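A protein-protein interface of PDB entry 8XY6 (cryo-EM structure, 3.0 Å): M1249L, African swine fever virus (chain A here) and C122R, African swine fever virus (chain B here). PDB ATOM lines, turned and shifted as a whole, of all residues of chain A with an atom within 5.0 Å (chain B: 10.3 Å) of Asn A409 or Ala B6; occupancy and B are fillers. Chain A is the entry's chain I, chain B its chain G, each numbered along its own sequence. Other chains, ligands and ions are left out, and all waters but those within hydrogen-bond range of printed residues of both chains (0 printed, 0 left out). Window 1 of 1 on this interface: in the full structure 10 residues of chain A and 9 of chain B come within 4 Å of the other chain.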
ATOM      1  N   ARG A 402      -0.684   4.784  10.072  1.00  0.00           N
ATOM      2  CA  ARG A 402      -0.083   4.996  11.382  1.00  0.00           C
ATOM      3  C   ARG A 402       0.290   6.452  11.594  1.00  0.00           C
ATOM      4  O   ARG A 402       0.072   6.997  12.677  1.00  0.00           O
ATOM      5  CB  ARG A 402       1.150   4.115  11.536  1.00  0.00           C
ATOM      6  CG  ARG A 402       1.695   4.074  12.940  1.00  0.00           C
ATOM      7  CD  ARG A 402       2.776   3.026  13.059  1.00  0.00           C
ATOM      8  NE  ARG A 402       2.442   1.785  12.370  1.00  0.00           N
ATOM      9  CZ  ARG A 402       1.479   0.952  12.741  1.00  0.00           C
ATOM     10  NH1 ARG A 402       0.721   1.199  13.795  1.00  0.00           N
ATOM     11  NH2 ARG A 402       1.274  -0.157  12.039  1.00  0.00           N
ATOM     12  N   PHE A 404      -1.047   9.030  10.128  1.00  0.00           N
ATOM     13  CA  PHE A 404      -2.290   9.778  10.274  1.00  0.00           C
ATOM     14  C   PHE A 404      -2.831   9.663  11.693  1.00  0.00           C
ATOM     15  O   PHE A 404      -3.179  10.670  12.317  1.00  0.00           O
ATOM     16  CB  PHE A 404      -3.326   9.290   9.266  1.00  0.00           C
ATOM     17  CG  PHE A 404      -4.640  10.008   9.358  1.00  0.00           C
ATOM     18  CD1 PHE A 404      -4.805  11.255   8.784  1.00  0.00           C
ATOM     19  CD2 PHE A 404      -5.712   9.436  10.017  1.00  0.00           C
ATOM     20  CE1 PHE A 404      -6.012  11.914   8.865  1.00  0.00           C
ATOM     21  CE2 PHE A 404      -6.920  10.093  10.102  1.00  0.00           C
ATOM     22  CZ  PHE A 404      -7.069  11.332   9.524  1.00  0.00           C
ATOM     23  N   LEU A 405      -2.896   8.439  12.223  1.00  0.00           N
ATOM     24  CA  LEU A 405      -3.418   8.249  13.574  1.00  0.00           C
ATOM     25  C   LEU A 405      -2.516   8.899  14.614  1.00  0.00           C
ATOM     26  O   LEU A 405      -2.999   9.447  15.610  1.00  0.00           O
ATOM     27  CB  LEU A 405      -3.588   6.763  13.876  1.00  0.00           C
ATOM     28  CG  LEU A 405      -4.521   5.985  12.956  1.00  0.00           C
ATOM     29  CD1 LEU A 405      -4.821   4.620  13.540  1.00  0.00           C
ATOM     30  CD2 LEU A 405      -5.794   6.757  12.710  1.00  0.00           C
ATOM     31  N   TYR A 406      -1.204   8.844  14.400  1.00  0.00           N
ATOM     32  CA  TYR A 406      -0.260   9.452  15.329  1.00  0.00           C
ATOM     33  C   TYR A 406      -0.470  10.956  15.409  1.00  0.00           C
ATOM     34  O   TYR A 406      -0.570  11.527  16.502  1.00  0.00           O
ATOM     35  CB  TYR A 406       1.167   9.126  14.886  1.00  0.00           C
ATOM     36  CG  TYR A 406       2.253   9.788  15.697  1.00  0.00           C
ATOM     37  CD1 TYR A 406       2.686   9.235  16.890  1.00  0.00           C
ATOM     38  CD2 TYR A 406       2.857  10.956  15.260  1.00  0.00           C
ATOM     39  CE1 TYR A 406       3.680   9.829  17.631  1.00  0.00           C
ATOM     40  CE2 TYR A 406       3.852  11.558  15.995  1.00  0.00           C
ATOM     41  CZ  TYR A 406       4.260  10.990  17.181  1.00  0.00           C
ATOM     42  OH  TYR A 406       5.254  11.585  17.921  1.00  0.00           O
ATOM     43  N   ASN A 407      -0.559  11.618  14.255  1.00  0.00           N
ATOM     44  CA  ASN A 407      -0.773  13.058  14.265  1.00  0.00           C
ATOM     45  C   ASN A 407      -2.160  13.415  14.778  1.00  0.00           C
ATOM     46  O   ASN A 407      -2.324  14.431  15.463  1.00  0.00           O
ATOM     47  CB  ASN A 407      -0.536  13.619  12.869  1.00  0.00           C
ATOM     48  CG  ASN A 407       0.898  13.453  12.425  1.00  0.00           C
ATOM     49  OD1 ASN A 407       1.825  13.639  13.210  1.00  0.00           O
ATOM     50  ND2 ASN A 407       1.091  13.079  11.169  1.00  0.00           N
ATOM     51  N   TYR A 408      -3.167  12.588  14.488  1.00  0.00           N
ATOM     52  CA  TYR A 408      -4.498  12.853  15.019  1.00  0.00           C
ATOM     53  C   TYR A 408      -4.517  12.769  16.538  1.00  0.00           C
ATOM     54  O   TYR A 408      -5.126  13.612  17.203  1.00  0.00           O
ATOM     55  CB  TYR A 408      -5.509  11.879  14.421  1.00  0.00           C
ATOM     56  CG  TYR A 408      -6.890  12.053  14.991  1.00  0.00           C
ATOM     57  CD1 TYR A 408      -7.531  13.281  14.938  1.00  0.00           C
ATOM     58  CD2 TYR A 408      -7.545  10.998  15.598  1.00  0.00           C
ATOM     59  CE1 TYR A 408      -8.792  13.450  15.462  1.00  0.00           C
ATOM     60  CE2 TYR A 408      -8.806  11.158  16.128  1.00  0.00           C
ATOM     61  CZ  TYR A 408      -9.426  12.384  16.057  1.00  0.00           C
ATOM     62  OH  TYR A 408     -10.686  12.543  16.583  1.00  0.00           O
ATOM     63  N   ASN A 409      -3.859  11.760  17.110  1.00  0.00           N
ATOM     64  CA  ASN A 409      -3.810  11.650  18.563  1.00  0.00           C
ATOM     65  C   ASN A 409      -2.923  12.722  19.179  1.00  0.00           C
ATOM     66  O   ASN A 409      -3.120  13.092  20.341  1.00  0.00           O
ATOM     67  CB  ASN A 409      -3.340  10.259  18.977  1.00  0.00           C
ATOM     68  CG  ASN A 409      -4.478   9.383  19.437  1.00  0.00           C
ATOM     69  OD1 ASN A 409      -4.771   9.304  20.627  1.00  0.00           O
ATOM     70  ND2 ASN A 409      -5.143   8.732  18.492  1.00  0.00           N
ATOM     71  N   CYS A 410      -1.937  13.220  18.434  1.00  0.00           N
ATOM     72  CA  CYS A 410      -1.230  14.411  18.887  1.00  0.00           C
ATOM     73  C   CYS A 410      -2.176  15.600  18.961  1.00  0.00           C
ATOM     74  O   CYS A 410      -2.119  16.395  19.905  1.00  0.00           O
ATOM     75  CB  CYS A 410      -0.053  14.711  17.963  1.00  0.00           C
ATOM     76  SG  CYS A 410       1.301  13.524  18.082  1.00  0.00           S
ATOM     77  N   LEU A 411      -3.059  15.734  17.970  1.00  0.00           N
ATOM     78  CA  LEU A 411      -4.058  16.798  17.998  1.00  0.00           C
ATOM     79  C   LEU A 411      -5.030  16.616  19.157  1.00  0.00           C
ATOM     80  O   LEU A 411      -5.474  17.596  19.765  1.00  0.00           O
ATOM     81  CB  LEU A 411      -4.813  16.842  16.670  1.00  0.00           C
ATOM     82  CG  LEU A 411      -6.174  17.543  16.657  1.00  0.00           C
ATOM     83  CD1 LEU A 411      -6.014  19.042  16.829  1.00  0.00           C
ATOM     84  CD2 LEU A 411      -6.933  17.226  15.382  1.00  0.00           C
ATOM     85  N   ARG A 412      -5.395  15.371  19.461  1.00  0.00           N
ATOM     86  CA  ARG A 412      -6.323  15.126  20.559  1.00  0.00           C
ATOM     87  C   ARG A 412      -5.687  15.441  21.906  1.00  0.00           C
ATOM     88  O   ARG A 412      -6.320  16.061  22.766  1.00  0.00           O
ATOM     89  CB  ARG A 412      -6.808  13.679  20.526  1.00  0.00           C
ATOM     90  CG  ARG A 412      -7.506  13.288  19.239  1.00  0.00           C
ATOM     91  CD  ARG A 412      -8.651  12.313  19.478  1.00  0.00           C
ATOM     92  NE  ARG A 412      -8.308  11.263  20.429  1.00  0.00           N
ATOM     93  CZ  ARG A 412      -8.765  11.203  21.672  1.00  0.00           C
ATOM     94  NH1 ARG A 412      -9.587  12.120  22.151  1.00  0.00           N
ATOM     95  NH2 ARG A 412      -8.387  10.196  22.454  1.00  0.00           N
ATOM     96  N   HIS A 413      -4.435  15.042  22.104  1.00  0.00           N
ATOM     97  CA  HIS A 413      -3.764  15.147  23.400  1.00  0.00           C
ATOM     98  C   HIS A 413      -2.835  16.352  23.485  1.00  0.00           C
ATOM     99  O   HIS A 413      -1.761  16.257  24.082  1.00  0.00           O
ATOM    100  CB  HIS A 413      -2.993  13.866  23.700  1.00  0.00           C
ATOM    101  CG  HIS A 413      -3.862  12.667  23.917  1.00  0.00           C
ATOM    102  ND1 HIS A 413      -4.127  11.751  22.923  1.00  0.00           N
ATOM    103  CD2 HIS A 413      -4.519  12.229  25.016  1.00  0.00           C
ATOM    104  CE1 HIS A 413      -4.915  10.803  23.400  1.00  0.00           C
ATOM    105  NE2 HIS A 413      -5.169  11.071  24.667  1.00  0.00           N
ATOM    106  N   VAL A 447      -9.077   5.197  15.819  1.00  0.00           N
ATOM    107  CA  VAL A 447      -8.295   3.990  15.570  1.00  0.00           C
ATOM    108  C   VAL A 447      -9.196   2.767  15.450  1.00  0.00           C
ATOM    109  O   VAL A 447      -8.893   1.840  14.689  1.00  0.00           O
ATOM    110  CB  VAL A 447      -7.230   3.808  16.667  1.00  0.00           C
ATOM    111  CG1 VAL A 447      -7.882   3.556  18.016  1.00  0.00           C
ATOM    112  CG2 VAL A 447      -6.287   2.673  16.310  1.00  0.00           C
ATOM    113  N   HIS A 451      -5.563  -2.105  13.910  1.00  0.00           N
ATOM    114  CA  HIS A 451      -4.323  -2.874  13.957  1.00  0.00           C
ATOM    115  C   HIS A 451      -4.591  -4.372  13.916  1.00  0.00           C
ATOM    116  O   HIS A 451      -3.974  -5.097  13.129  1.00  0.00           O
ATOM    117  CB  HIS A 451      -3.526  -2.494  15.200  1.00  0.00           C
ATOM    118  CG  HIS A 451      -2.991  -1.099  15.155  1.00  0.00           C
ATOM    119  ND1 HIS A 451      -3.335  -0.140  16.083  1.00  0.00           N
ATOM    120  CD2 HIS A 451      -2.152  -0.495  14.282  1.00  0.00           C
ATOM    121  CE1 HIS A 451      -2.722   0.992  15.788  1.00  0.00           C
ATOM    122  NE2 HIS A 451      -1.999   0.803  14.699  1.00  0.00           N
ATOM    123  N   LYS B   2       4.076  -2.875  26.636  1.00  0.00           N
ATOM    124  CA  LYS B   2       2.983  -1.927  26.478  1.00  0.00           C
ATOM    125  C   LYS B   2       3.202  -1.146  25.191  1.00  0.00           C
ATOM    126  O   LYS B   2       4.216  -0.456  25.042  1.00  0.00           O
ATOM    127  CB  LYS B   2       2.885  -0.984  27.676  1.00  0.00           C
ATOM    128  CG  LYS B   2       1.453  -0.621  28.035  1.00  0.00           C
ATOM    129  CD  LYS B   2       0.699  -1.843  28.532  1.00  0.00           C
ATOM    130  CE  LYS B   2      -0.797  -1.599  28.564  1.00  0.00           C
ATOM    131  NZ  LYS B   2      -1.407  -1.778  27.220  1.00  0.00           N
ATOM    132  N   ILE B   3       2.259  -1.270  24.264  1.00  0.00           N
ATOM    133  CA  ILE B   3       2.281  -0.544  23.002  1.00  0.00           C
ATOM    134  C   ILE B   3       1.098   0.414  22.959  1.00  0.00           C
ATOM    135  O   ILE B   3       0.037   0.139  23.529  1.00  0.00           O
ATOM    136  CB  ILE B   3       2.314  -1.505  21.790  1.00  0.00           C
ATOM    137  CG1 ILE B   3       1.374  -2.722  21.930  1.00  0.00           C
ATOM    138  CG2 ILE B   3       3.740  -1.971  21.519  1.00  0.00           C
ATOM    139  CD1 ILE B   3      -0.097  -2.469  22.160  1.00  0.00           C
ATOM    140  N   CYS B   4       1.306   1.571  22.338  1.00  0.00           N
ATOM    141  CA  CYS B   4       0.235   2.548  22.233  1.00  0.00           C
ATOM    142  C   CYS B   4      -0.842   2.029  21.295  1.00  0.00           C
ATOM    143  O   CYS B   4      -0.551   1.573  20.188  1.00  0.00           O
ATOM    144  CB  CYS B   4       0.780   3.884  21.736  1.00  0.00           C
ATOM    145  SG  CYS B   4      -0.502   5.066  21.314  1.00  0.00           S
ATOM    146  N   LYS B   5      -2.095   2.098  21.743  1.00  0.00           N
ATOM    147  CA  LYS B   5      -3.184   1.536  20.953  1.00  0.00           C
ATOM    148  C   LYS B   5      -3.347   2.275  19.632  1.00  0.00           C
ATOM    149  O   LYS B   5      -3.645   1.660  18.602  1.00  0.00           O
ATOM    150  CB  LYS B   5      -4.480   1.572  21.756  1.00  0.00           C
ATOM    151  CG  LYS B   5      -5.294   0.299  21.660  1.00  0.00           C
ATOM    152  CD  LYS B   5      -4.684  -0.797  22.512  1.00  0.00           C
ATOM    153  CE  LYS B   5      -5.522  -2.062  22.466  1.00  0.00           C
ATOM    154  NZ  LYS B   5      -4.857  -3.187  23.174  1.00  0.00           N
ATOM    155  N   ALA B   6      -3.160   3.595  19.642  1.00  0.00           N
ATOM    156  CA  ALA B   6      -3.405   4.382  18.439  1.00  0.00           C
ATOM    157  C   ALA B   6      -2.299   4.208  17.405  1.00  0.00           C
ATOM    158  O   ALA B   6      -2.581   4.024  16.217  1.00  0.00           O
ATOM    159  CB  ALA B   6      -3.565   5.856  18.806  1.00  0.00           C
ATOM    160  N   CYS B   7      -1.036   4.260  17.829  1.00  0.00           N
ATOM    161  CA  CYS B   7       0.069   4.310  16.880  1.00  0.00           C
ATOM    162  C   CYS B   7       1.069   3.171  17.046  1.00  0.00           C
ATOM    163  O   CYS B   7       2.110   3.184  16.379  1.00  0.00           O
ATOM    164  CB  CYS B   7       0.796   5.655  16.979  1.00  0.00           C
ATOM    165  SG  CYS B   7       1.829   5.851  18.440  1.00  0.00           S
ATOM    166  N   SER B   8       0.785   2.193  17.908  1.00  0.00           N
ATOM    167  CA  SER B   8       1.614   0.996  18.054  1.00  0.00           C
ATOM    168  C   SER B   8       3.081   1.332  18.294  1.00  0.00           C
ATOM    169  O   SER B   8       3.968   0.767  17.653  1.00  0.00           O
ATOM    170  CB  SER B   8       1.472   0.073  16.843  1.00  0.00           C
ATOM    171  OG  SER B   8       0.145  -0.404  16.724  1.00  0.00           O
ATOM    172  N   SER B   9       3.352   2.256  19.203  1.00  0.00           N
ATOM    173  CA  SER B   9       4.715   2.615  19.554  1.00  0.00           C
ATOM    174  C   SER B   9       5.010   2.216  20.993  1.00  0.00           C
ATOM    175  O   SER B   9       4.105   1.958  21.790  1.00  0.00           O
ATOM    176  CB  SER B   9       4.950   4.115  19.361  1.00  0.00           C
ATOM    177  OG  SER B   9       6.335   4.419  19.343  1.00  0.00           O
ATOM    178  N   CYS B  10       6.298   2.160  21.317  1.00  0.00           N
ATOM    179  CA  CYS B  10       6.714   1.804  22.667  1.00  0.00           C
ATOM    180  C   CYS B  10       6.375   2.923  23.644  1.00  0.00           C
ATOM    181  O   CYS B  10       6.648   4.099  23.390  1.00  0.00           O
ATOM    182  CB  CYS B  10       8.211   1.513  22.700  1.00  0.00           C
ATOM    183  SG  CYS B  10       8.738   0.201  21.582  1.00  0.00           S
ATOM    184  N   MET B  11       5.782   2.548  24.774  1.00  0.00           N
ATOM    185  CA  MET B  11       5.327   3.493  25.782  1.00  0.00           C
ATOM    186  C   MET B  11       6.169   3.346  27.040  1.00  0.00           C
ATOM    187  O   MET B  11       6.219   2.266  27.636  1.00  0.00           O
ATOM    188  CB  MET B  11       3.852   3.268  26.109  1.00  0.00           C
ATOM    189  CG  MET B  11       2.898   3.775  25.052  1.00  0.00           C
ATOM    190  SD  MET B  11       1.334   4.316  25.756  1.00  0.00           S
ATOM    191  CE  MET B  11       0.513   2.741  25.964  1.00  0.00           C
ATOM    192  N   ARG B  23       3.055   6.225  29.116  1.00  0.00           N
ATOM    193  CA  ARG B  23       2.856   7.414  28.304  1.00  0.00           C
ATOM    194  C   ARG B  23       3.585   7.263  26.979  1.00  0.00           C
ATOM    195  O   ARG B  23       4.777   6.943  26.946  1.00  0.00           O
ATOM    196  CB  ARG B  23       3.346   8.666  29.035  1.00  0.00           C
ATOM    197  CG  ARG B  23       2.687   9.944  28.562  1.00  0.00           C
ATOM    198  CD  ARG B  23       3.593  11.144  28.754  1.00  0.00           C
ATOM    199  NE  ARG B  23       3.228  12.229  27.852  1.00  0.00           N
ATOM    200  CZ  ARG B  23       3.722  12.384  26.632  1.00  0.00           C
ATOM    201  NH1 ARG B  23       4.625  11.552  26.141  1.00  0.00           N
ATOM    202  NH2 ARG B  23       3.298  13.399  25.886  1.00  0.00           N
ATOM    203  N   CYS B  24       2.868   7.501  25.890  1.00  0.00           N
ATOM    204  CA  CYS B  24       3.428   7.406  24.552  1.00  0.00           C
ATOM    205  C   CYS B  24       4.035   8.741  24.138  1.00  0.00           C
ATOM    206  O   CYS B  24       3.959   9.739  24.856  1.00  0.00           O
ATOM    207  CB  CYS B  24       2.357   6.979  23.549  1.00  0.00           C
ATOM    208  SG  CYS B  24       2.995   6.668  21.895  1.00  0.00           S
ATOM    209  N   SER B  25       4.656   8.744  22.958  1.00  0.00           N
ATOM    210  CA  SER B  25       5.158   9.995  22.407  1.00  0.00           C
ATOM    211  C   SER B  25       4.057  10.795  21.726  1.00  0.00           C
ATOM    212  O   SER B  25       4.268  11.968  21.405  1.00  0.00           O
ATOM    213  CB  SER B  25       6.296   9.726  21.424  1.00  0.00           C
ATOM    214  OG  SER B  25       6.696  10.918  20.771  1.00  0.00           O
ATOM    215  N   CYS B  26       2.898  10.184  21.492  1.00  0.00           N
ATOM    216  CA  CYS B  26       1.741  10.885  20.960  1.00  0.00           C
ATOM    217  C   CYS B  26       0.762  11.304  22.047  1.00  0.00           C
ATOM    218  O   CYS B  26      -0.294  11.861  21.734  1.00  0.00           O
ATOM    219  CB  CYS B  26       1.030  10.019  19.918  1.00  0.00           C
ATOM    220  SG  CYS B  26       0.093   8.637  20.584  1.00  0.00           S
ATOM    221  N   GLY B  27       1.086  11.045  23.313  1.00  0.00           N
ATOM    222  CA  GLY B  27       0.291  11.516  24.424  1.00  0.00           C
ATOM    223  C   GLY B  27      -0.633  10.494  25.049  1.00  0.00           C
ATOM    224  O   GLY B  27      -1.151  10.745  26.144  1.00  0.00           O
ATOM    225  N   GLU B  28      -0.858   9.355  24.402  1.00  0.00           N
ATOM    226  CA  GLU B  28      -1.795   8.377  24.934  1.00  0.00           C
ATOM    227  C   GLU B  28      -1.268   7.770  26.228  1.00  0.00           C
ATOM    228  O   GLU B  28      -0.082   7.452  26.350  1.00  0.00           O
ATOM    229  CB  GLU B  28      -2.059   7.280  23.906  1.00  0.00           C
ATOM    230  CG  GLU B  28      -3.257   6.411  24.233  1.00  0.00           C
ATOM    231  CD  GLU B  28      -4.516   6.860  23.517  1.00  0.00           C
ATOM    232  OE1 GLU B  28      -4.764   6.385  22.390  1.00  0.00           O
ATOM    233  OE2 GLU B  28      -5.256   7.693  24.080  1.00  0.00           O
ATOM    234  N   SER B  29      -2.161   7.619  27.204  1.00  0.00           N
ATOM    235  CA  SER B  29      -1.845   7.018  28.492  1.00  0.00           C
ATOM    236  C   SER B  29      -2.870   5.934  28.792  1.00  0.00           C
ATOM    237  O   SER B  29      -4.061   6.109  28.525  1.00  0.00           O
ATOM    238  CB  SER B  29      -1.831   8.064  29.607  1.00  0.00           C
ATOM    239  OG  SER B  29      -0.977   9.146  29.273  1.00  0.00           O
ATOM    240  N   VAL B  30      -2.406   4.819  29.351  1.00  0.00           N
ATOM    241  CA  VAL B  30      -3.238   3.624  29.426  1.00  0.00           C
ATOM    242  C   VAL B  30      -3.279   3.095  30.857  1.00  0.00           C
ATOM    243  O   VAL B  30      -3.848   2.030  31.121  1.00  0.00           O
ATOM    244  CB  VAL B  30      -2.721   2.554  28.446  1.00  0.00           C
ATOM    245  CG1 VAL B  30      -1.382   2.005  28.916  1.00  0.00           C
ATOM    246  CG2 VAL B  30      -3.758   1.451  28.200  1.00  0.00           C
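Printed residues of chain B within 4 Å of Asn A409: Ala B6 (3.3 Å), Cys B26 (3.4 Å) and Glu B28 (3.4 Å).
Of chain A, only Leu A405, Asn A409, Val A447 and His A451 come within 4 Å of Ala B6.
Leu A405 touches just one residue of chain B: Ala B6.
No residue of chain B comes within 4 Å of Arg A412.
Of the printed residues of chain B, His A413 touches Cys B26, Gly B27 and Glu B28.
Of the printed residues of chain B, Arg A402 touches Cys B7 and Ser B8.
Of the printed residues of chain A, Glu B28 touches Asn A409 and His A413.
Ile B3 touches none of the printed residues of chain A.
The nearest residue of chain B that does not touch Asn A409 is Gly B27 (5.5 Å).
Hydrophobic or aromatic side chains of chain A within 4 Å of the printed part of chain B: Leu A405, Tyr A406, His A413, Val A447 and His A451.
Among the printed residues, no Asp or Glu carboxylate lies within 4 Å of a Lys or Arg side-chain nitrogen of the other chain.
O of Cys B7 touches CD of Arg A402 (3.4 Å).
Leu A405 touches Ala B6.
CD1 of Tyr A406 touches SG of Cys B7 (3.8 Å).
CB of Cys B26 touches CE1 of Tyr A406, 3.5 Å away.
Ala B6 touches Asn A409 (CB to ND2, 3.3 Å).
Cys A410 touches Cys B26 (N to O, 3.9 Å).
CB of His A413 touches O of Cys B26, at 3.9 Å.
His A413 touches Gly B27.
O of Ala B6 touches CG2 of Val A447 (3.9 Å).
His A451 touches Ala B6 (CE1 to O, 3.1 Å).
The backbone carbonyl oxygen (O) of Tyr A406 sits at hydrogen-bond distance from the side-chain sulfur (SG) of Cys A410 (3.2 Å).
N of Ala B6 lies close to SG of Cys B4, 3.5 Å away.
O of Asn A409 lies within hydrogen-bond range of ND1 of His A413 (3.1 Å).
The guanidinium group (NH1) of Arg A402 sits at hydrogen-bond distance from a ring nitrogen (NE2) of His A451, 2.9 Å away.
A ring nitrogen (NE2) of His A413 lies close to the side-chain carboxylate of Glu B28 (3.4 Å).
The side-chain hydroxyl (OG) of Ser B8 lies close to the guanidinium group (NH1) of Arg A402 (3.4 Å).
OE1 of Glu B28 lies close to OD1 of Asn A409.
O of Lys B5 lies close to ND1 of His A451 (3.1 Å).
OG of Ser B8 sits at hydrogen-bond distance from NE2 of His A451.
O of Asn A409 sits close to O of Cys B26 (3.4 Å).
OG of Ser B25 is in hydrogen-bond range of OH of Tyr A406, 3.3 Å away.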
